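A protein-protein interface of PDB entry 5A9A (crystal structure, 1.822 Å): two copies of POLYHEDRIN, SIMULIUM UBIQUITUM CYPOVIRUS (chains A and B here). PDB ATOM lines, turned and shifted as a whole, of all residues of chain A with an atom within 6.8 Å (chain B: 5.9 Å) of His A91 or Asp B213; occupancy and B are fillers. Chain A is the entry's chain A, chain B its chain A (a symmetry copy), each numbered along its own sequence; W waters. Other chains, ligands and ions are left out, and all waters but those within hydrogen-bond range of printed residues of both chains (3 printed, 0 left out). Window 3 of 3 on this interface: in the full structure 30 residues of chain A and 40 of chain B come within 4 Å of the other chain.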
ATOM      1  N   LYS A  80       4.891  24.182  21.694  1.00  0.00           N
ATOM      2  CA  LYS A  80       3.489  23.869  21.447  1.00  0.00           C
ATOM      3  C   LYS A  80       3.328  22.429  20.968  1.00  0.00           C
ATOM      4  O   LYS A  80       2.474  21.692  21.463  1.00  0.00           O
ATOM      5  CB  LYS A  80       2.888  24.815  20.408  1.00  0.00           C
ATOM      6  CG  LYS A  80       1.445  24.477  20.050  1.00  0.00           C
ATOM      7  CD  LYS A  80       0.863  25.458  19.050  1.00  0.00           C
ATOM      8  CE  LYS A  80       1.354  25.182  17.640  1.00  0.00           C
ATOM      9  NZ  LYS A  80       0.857  26.206  16.681  1.00  0.00           N
ATOM     10  N   GLU A  81       4.146  22.033  19.996  1.00  0.00           N
ATOM     11  CA  GLU A  81       4.032  20.706  19.405  1.00  0.00           C
ATOM     12  C   GLU A  81       4.415  19.625  20.407  1.00  0.00           C
ATOM     13  O   GLU A  81       3.790  18.566  20.462  1.00  0.00           O
ATOM     14  CB  GLU A  81       4.906  20.592  18.157  1.00  0.00           C
ATOM     15  CG  GLU A  81       4.504  21.531  17.037  1.00  0.00           C
ATOM     16  CD  GLU A  81       3.055  21.354  16.623  1.00  0.00           C
ATOM     17  OE1 GLU A  81       2.456  20.305  16.953  1.00  0.00           O
ATOM     18  OE2 GLU A  81       2.515  22.265  15.965  1.00  0.00           O
ATOM     19  N   ASN A  84       1.544  19.235  22.684  1.00  0.00           N
ATOM     20  CA  ASN A  84       0.503  18.456  22.021  1.00  0.00           C
ATOM     21  C   ASN A  84       0.753  16.962  22.168  1.00  0.00           C
ATOM     22  O   ASN A  84      -0.125  16.211  22.598  1.00  0.00           O
ATOM     23  CB  ASN A  84       0.421  18.801  20.534  1.00  0.00           C
ATOM     24  CG  ASN A  84      -0.396  20.047  20.262  1.00  0.00           C
ATOM     25  OD1 ASN A  84      -1.260  20.424  21.054  1.00  0.00           O
ATOM     26  ND2 ASN A  84      -0.137  20.688  19.124  1.00  0.00           N
ATOM     27  N   GLN A  85       1.956  16.533  21.805  1.00  0.00           N
ATOM     28  CA  GLN A  85       2.301  15.119  21.843  1.00  0.00           C
ATOM     29  C   GLN A  85       2.195  14.567  23.262  1.00  0.00           C
ATOM     30  O   GLN A  85       1.741  13.442  23.466  1.00  0.00           O
ATOM     31  CB  GLN A  85       3.712  14.897  21.294  1.00  0.00           C
ATOM     32  CG  GLN A  85       4.095  13.431  21.182  1.00  0.00           C
ATOM     33  CD  GLN A  85       3.051  12.616  20.439  1.00  0.00           C
ATOM     34  OE1 GLN A  85       2.377  13.118  19.541  1.00  0.00           O
ATOM     35  NE2 GLN A  85       2.907  11.354  20.818  1.00  0.00           N
ATOM     36  N   ARG A  88      -1.760  15.203  24.426  1.00  0.00           N
ATOM     37  CA  ARG A  88      -2.742  14.624  23.519  1.00  0.00           C
ATOM     38  C   ARG A  88      -2.059  13.877  22.376  1.00  0.00           C
ATOM     39  O   ARG A  88      -2.096  14.310  21.222  1.00  0.00           O
ATOM     40  CB  ARG A  88      -3.702  15.696  22.983  1.00  0.00           C
ATOM     41  CG  ARG A  88      -3.069  17.040  22.666  1.00  0.00           C
ATOM     42  CD  ARG A  88      -4.129  18.048  22.224  1.00  0.00           C
ATOM     43  NE  ARG A  88      -4.817  17.628  21.003  1.00  0.00           N
ATOM     44  CZ  ARG A  88      -4.533  18.074  19.783  1.00  0.00           C
ATOM     45  NH1 ARG A  88      -3.576  18.973  19.600  1.00  0.00           N
ATOM     46  NH2 ARG A  88      -5.218  17.625  18.741  1.00  0.00           N
ATOM     47  N   PRO A  89      -1.428  12.741  22.700  1.00  0.00           N
ATOM     48  CA  PRO A  89      -0.809  11.874  21.693  1.00  0.00           C
ATOM     49  C   PRO A  89      -1.863  11.311  20.747  1.00  0.00           C
ATOM     50  O   PRO A  89      -2.961  11.008  21.213  1.00  0.00           O
ATOM     51  CB  PRO A  89      -0.189  10.750  22.531  1.00  0.00           C
ATOM     52  CG  PRO A  89      -0.958  10.757  23.808  1.00  0.00           C
ATOM     53  CD  PRO A  89      -1.288  12.193  24.058  1.00  0.00           C
ATOM     54  N   ASP A  90      -1.566  11.185  19.455  1.00  0.00           N
ATOM     55  CA  ASP A  90      -0.288  11.590  18.871  1.00  0.00           C
ATOM     56  C   ASP A  90      -0.496  12.803  17.966  1.00  0.00           C
ATOM     57  O   ASP A  90      -0.303  12.720  16.752  1.00  0.00           O
ATOM     58  CB  ASP A  90       0.289  10.440  18.044  1.00  0.00           C
ATOM     59  CG  ASP A  90       0.521   9.187  18.867  1.00  0.00           C
ATOM     60  OD1 ASP A  90       1.224   9.273  19.898  1.00  0.00           O
ATOM     61  OD2 ASP A  90      -0.008   8.119  18.488  1.00  0.00           O
ATOM     62  N   HIS A  91      -0.882  13.931  18.554  1.00  0.00           N
ATOM     63  CA  HIS A  91      -1.304  15.084  17.761  1.00  0.00           C
ATOM     64  C   HIS A  91      -0.287  16.222  17.707  1.00  0.00           C
ATOM     65  O   HIS A  91      -0.629  17.343  17.329  1.00  0.00           O
ATOM     66  CB  HIS A  91      -2.635  15.618  18.289  1.00  0.00           C
ATOM     67  CG  HIS A  91      -3.762  14.641  18.173  1.00  0.00           C
ATOM     68  ND1 HIS A  91      -4.057  13.723  19.157  1.00  0.00           N
ATOM     69  CD2 HIS A  91      -4.661  14.434  17.182  1.00  0.00           C
ATOM     70  CE1 HIS A  91      -5.097  12.999  18.782  1.00  0.00           C
ATOM     71  NE2 HIS A  91      -5.479  13.406  17.585  1.00  0.00           N
ATOM     72  N   GLY A  92       0.957  15.938  18.072  1.00  0.00           N
ATOM     73  CA  GLY A  92       2.001  16.946  18.018  1.00  0.00           C
ATOM     74  C   GLY A  92       2.991  16.699  16.897  1.00  0.00           C
ATOM     75  O   GLY A  92       3.515  15.596  16.754  1.00  0.00           O
ATOM     76  N   ASP A  93       3.244  17.727  16.094  1.00  0.00           N
ATOM     77  CA  ASP A  93       4.293  17.657  15.087  1.00  0.00           C
ATOM     78  C   ASP A  93       5.631  17.847  15.797  1.00  0.00           C
ATOM     79  O   ASP A  93       6.317  18.852  15.615  1.00  0.00           O
ATOM     80  CB  ASP A  93       4.085  18.720  14.005  1.00  0.00           C
ATOM     81  CG  ASP A  93       5.008  18.533  12.819  1.00  0.00           C
ATOM     82  OD1 ASP A  93       5.661  17.472  12.734  1.00  0.00           O
ATOM     83  OD2 ASP A  93       5.075  19.444  11.967  1.00  0.00           O
ATOM     84  N   SER A  94       5.980  16.862  16.618  1.00  0.00           N
ATOM     85  CA  SER A  94       7.158  16.927  17.473  1.00  0.00           C
ATOM     86  C   SER A  94       8.072  15.747  17.157  1.00  0.00           C
ATOM     87  O   SER A  94       7.609  14.612  17.067  1.00  0.00           O
ATOM     88  CB  SER A  94       6.720  16.905  18.941  1.00  0.00           C
ATOM     89  OG  SER A  94       7.826  16.820  19.820  1.00  0.00           O
ATOM     90  N   LEU B 208      -6.267  22.631  18.712  1.00  0.00           N
ATOM     91  CA  LEU B 208      -6.741  21.457  17.991  1.00  0.00           C
ATOM     92  C   LEU B 208      -7.260  21.882  16.617  1.00  0.00           C
ATOM     93  O   LEU B 208      -8.113  22.764  16.512  1.00  0.00           O
ATOM     94  CB  LEU B 208      -7.839  20.746  18.792  1.00  0.00           C
ATOM     95  CG  LEU B 208      -7.460  20.269  20.202  1.00  0.00           C
ATOM     96  CD1 LEU B 208      -7.620  21.377  21.236  1.00  0.00           C
ATOM     97  CD2 LEU B 208      -8.296  19.062  20.606  1.00  0.00           C
ATOM     98  N   ASP B 209      -6.740  21.250  15.569  1.00  0.00           N
ATOM     99  CA  ASP B 209      -6.995  21.687  14.196  1.00  0.00           C
ATOM    100  C   ASP B 209      -8.459  21.584  13.771  1.00  0.00           C
ATOM    101  O   ASP B 209      -8.990  22.488  13.124  1.00  0.00           O
ATOM    102  CB  ASP B 209      -6.152  20.875  13.213  1.00  0.00           C
ATOM    103  CG  ASP B 209      -4.678  21.210  13.287  1.00  0.00           C
ATOM    104  OD1 ASP B 209      -4.315  22.191  13.969  1.00  0.00           O
ATOM    105  OD2 ASP B 209      -3.884  20.492  12.646  1.00  0.00           O
ATOM    106  N   ASN B 210      -9.104  20.477  14.122  1.00  0.00           N
ATOM    107  CA  ASN B 210     -10.432  20.175  13.601  1.00  0.00           C
ATOM    108  C   ASN B 210     -11.275  19.405  14.610  1.00  0.00           C
ATOM    109  O   ASN B 210     -10.787  19.016  15.670  1.00  0.00           O
ATOM    110  CB  ASN B 210     -10.306  19.373  12.306  1.00  0.00           C
ATOM    111  CG  ASN B 210      -9.626  18.038  12.517  1.00  0.00           C
ATOM    112  OD1 ASN B 210     -10.251  17.081  12.969  1.00  0.00           O
ATOM    113  ND2 ASN B 210      -8.337  17.968  12.193  1.00  0.00           N
ATOM    114  N   GLU B 211     -12.542  19.176  14.281  1.00  0.00           N
ATOM    115  CA  GLU B 211     -13.462  18.577  15.245  1.00  0.00           C
ATOM    116  C   GLU B 211     -13.193  17.091  15.468  1.00  0.00           C
ATOM    117  O   GLU B 211     -13.526  16.551  16.522  1.00  0.00           O
ATOM    118  CB  GLU B 211     -14.918  18.785  14.828  1.00  0.00           C
ATOM    119  CG  GLU B 211     -15.896  18.344  15.907  1.00  0.00           C
ATOM    120  CD  GLU B 211     -17.338  18.700  15.595  1.00  0.00           C
ATOM    121  OE1 GLU B 211     -17.676  18.863  14.405  1.00  0.00           O
ATOM    122  OE2 GLU B 211     -18.132  18.817  16.551  1.00  0.00           O
ATOM    123  N   GLY B 212     -12.595  16.430  14.483  1.00  0.00           N
ATOM    124  CA  GLY B 212     -12.218  15.037  14.637  1.00  0.00           C
ATOM    125  C   GLY B 212     -11.186  14.880  15.735  1.00  0.00           C
ATOM    126  O   GLY B 212     -11.303  14.004  16.593  1.00  0.00           O
ATOM    127  N   ASP B 213     -10.169  15.735  15.707  1.00  0.00           N
ATOM    128  CA  ASP B 213      -9.130  15.735  16.728  1.00  0.00           C
ATOM    129  C   ASP B 213      -9.715  16.104  18.091  1.00  0.00           C
ATOM    130  O   ASP B 213      -9.273  15.605  19.128  1.00  0.00           O
ATOM    131  CB  ASP B 213      -8.023  16.725  16.354  1.00  0.00           C
ATOM    132  CG  ASP B 213      -7.246  16.292  15.119  1.00  0.00           C
ATOM    133  OD1 ASP B 213      -7.662  15.311  14.468  1.00  0.00           O
ATOM    134  OD2 ASP B 213      -6.227  16.936  14.792  1.00  0.00           O
ATOM    135  N   LEU B 214     -10.710  16.986  18.084  1.00  0.00           N
ATOM    136  CA  LEU B 214     -11.350  17.423  19.319  1.00  0.00           C
ATOM    137  C   LEU B 214     -12.171  16.296  19.943  1.00  0.00           C
ATOM    138  O   LEU B 214     -12.080  16.046  21.144  1.00  0.00           O
ATOM    139  CB  LEU B 214     -12.238  18.640  19.058  1.00  0.00           C
ATOM    140  CG  LEU B 214     -13.049  19.154  20.251  1.00  0.00           C
ATOM    141  CD1 LEU B 214     -12.148  19.433  21.449  1.00  0.00           C
ATOM    142  CD2 LEU B 214     -13.821  20.401  19.859  1.00  0.00           C
ATOM    143  N   ILE B 215     -12.971  15.618  19.126  1.00  0.00           N
ATOM    144  CA  ILE B 215     -13.761  14.490  19.611  1.00  0.00           C
ATOM    145  C   ILE B 215     -12.832  13.448  20.221  1.00  0.00           C
ATOM    146  O   ILE B 215     -13.119  12.884  21.278  1.00  0.00           O
ATOM    147  CB  ILE B 215     -14.580  13.833  18.484  1.00  0.00           C
ATOM    148  CG1 ILE B 215     -15.646  14.798  17.961  1.00  0.00           C
ATOM    149  CG2 ILE B 215     -15.252  12.568  18.986  1.00  0.00           C
ATOM    150  CD1 ILE B 215     -16.369  14.295  16.723  1.00  0.00           C
ATOM    151  N   ASP B 216     -11.716  13.201  19.546  1.00  0.00           N
ATOM    152  CA  ASP B 216     -10.717  12.252  20.027  1.00  0.00           C
ATOM    153  C   ASP B 216     -10.203  12.646  21.415  1.00  0.00           C
ATOM    154  O   ASP B 216     -10.084  11.802  22.308  1.00  0.00           O
ATOM    155  CB  ASP B 216      -9.557  12.168  19.028  1.00  0.00           C
ATOM    156  CG  ASP B 216      -8.596  11.038  19.335  1.00  0.00           C
ATOM    157  OD1 ASP B 216      -7.684  11.237  20.164  1.00  0.00           O
ATOM    158  OD2 ASP B 216      -8.742   9.951  18.736  1.00  0.00           O
ATOM    159  N   TYR B 217      -9.904  13.931  21.595  1.00  0.00           N
ATOM    160  CA  TYR B 217      -9.420  14.440  22.880  1.00  0.00           C
ATOM    161  C   TYR B 217     -10.459  14.245  23.981  1.00  0.00           C
ATOM    162  O   TYR B 217     -10.150  13.752  25.065  1.00  0.00           O
ATOM    163  CB  TYR B 217      -9.072  15.925  22.761  1.00  0.00           C
ATOM    164  CG  TYR B 217      -8.556  16.556  24.042  1.00  0.00           C
ATOM    165  CD1 TYR B 217      -7.200  16.543  24.349  1.00  0.00           C
ATOM    166  CD2 TYR B 217      -9.422  17.181  24.932  1.00  0.00           C
ATOM    167  CE1 TYR B 217      -6.723  17.125  25.512  1.00  0.00           C
ATOM    168  CE2 TYR B 217      -8.955  17.762  26.098  1.00  0.00           C
ATOM    169  CZ  TYR B 217      -7.606  17.733  26.381  1.00  0.00           C
ATOM    170  OH  TYR B 217      -7.132  18.312  27.538  1.00  0.00           O
ATOM    171  N   MET B 218     -11.694  14.638  23.698  1.00  0.00           N
ATOM    172  CA  MET B 218     -12.756  14.565  24.693  1.00  0.00           C
ATOM    173  C   MET B 218     -13.014  13.113  25.103  1.00  0.00           C
ATOM    174  O   MET B 218     -13.254  12.817  26.273  1.00  0.00           O
ATOM    175  CB  MET B 218     -14.030  15.221  24.157  1.00  0.00           C
ATOM    176  CG  MET B 218     -13.848  16.696  23.806  1.00  0.00           C
ATOM    177  SD  MET B 218     -13.306  17.703  25.207  1.00  0.00           S
ATOM    178  CE  MET B 218     -14.819  17.778  26.172  1.00  0.00           C
HETATM  179  O   HOH W   1      -5.031  18.953  16.192  1.00  0.00           O
HETATM  180  O   HOH W   2      -6.455  13.292  21.637  1.00  0.00           O
HETATM  181  O   HOH W   3      -6.801  15.526  20.098  1.00  0.00           O
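The backbone carbonyl oxygen (O) of Arg A88 sits at hydrogen-bond distance from a ring nitrogen (ND1) of His A91, 2.9 Å away. OD1 of Asn A84 is in hydrogen-bond range of NH1 of Arg A88, 3.1 Å away. The side-chain amide oxygen of Asn B210 is in hydrogen-bond range of the backbone NH of Asp B213, at 3.1 Å.
Among the printed residues, merely in contact across the chains: Arg A88 with Leu B208 (3.7 Å), Arg A88 with Asp B213 (3.8 Å), Arg A88 with Tyr B217 (3.8 Å), His A91 with Asp B213 (3.8 Å) and His A91 with Asp B216 (3.4 Å).
His A91 touches just these residues of chain B: Asp B213 (3.8 Å) and Asp B216 (3.4 Å). Of chain A, only Arg A88 and His A91 come within 4 Å of Asp B213. Printed residues of chain A within 4 Å of Leu B208: Arg A88. Printed residues of chain A within 4 Å of Asp B216: His A91 (3.4 Å). Of the printed residues of chain A, Tyr B217 touches Arg A88 (3.8 Å). Asp B209 touches none of the printed residues of chain A. Met B218 touches none of the printed residues of chain A. The nearest printed residue of chain A that does not touch Leu B208 is Asn A84 (6.0 Å).
Of the 11 printed residues of chain B, 4 touch a printed residue of chain A. Hydrophobic or aromatic side chains of chain B within 4 Å of the printed part of chain A: Leu B208 and Tyr B217. Of the 11 printed residues of chain A, 2 touch a printed residue of chain B.
No position is printed for both chains.
Water W3 lies within hydrogen-bond range of the backbone carbonyl oxygen of Asp B213 (2.7 Å), the guanidinium group of Arg A88 (3.0 Å) and a ring nitrogen (ND1) of His A91 (3.4 Å). Water W1 lies within hydrogen-bond range of OD2 of Asp B213, NH2 of Arg A88 and N of Asp B209. Water W2 lies within hydrogen-bond range of OD1 of Asp B216 (2.8 Å) and ND1 of His A91 (3.5 Å).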
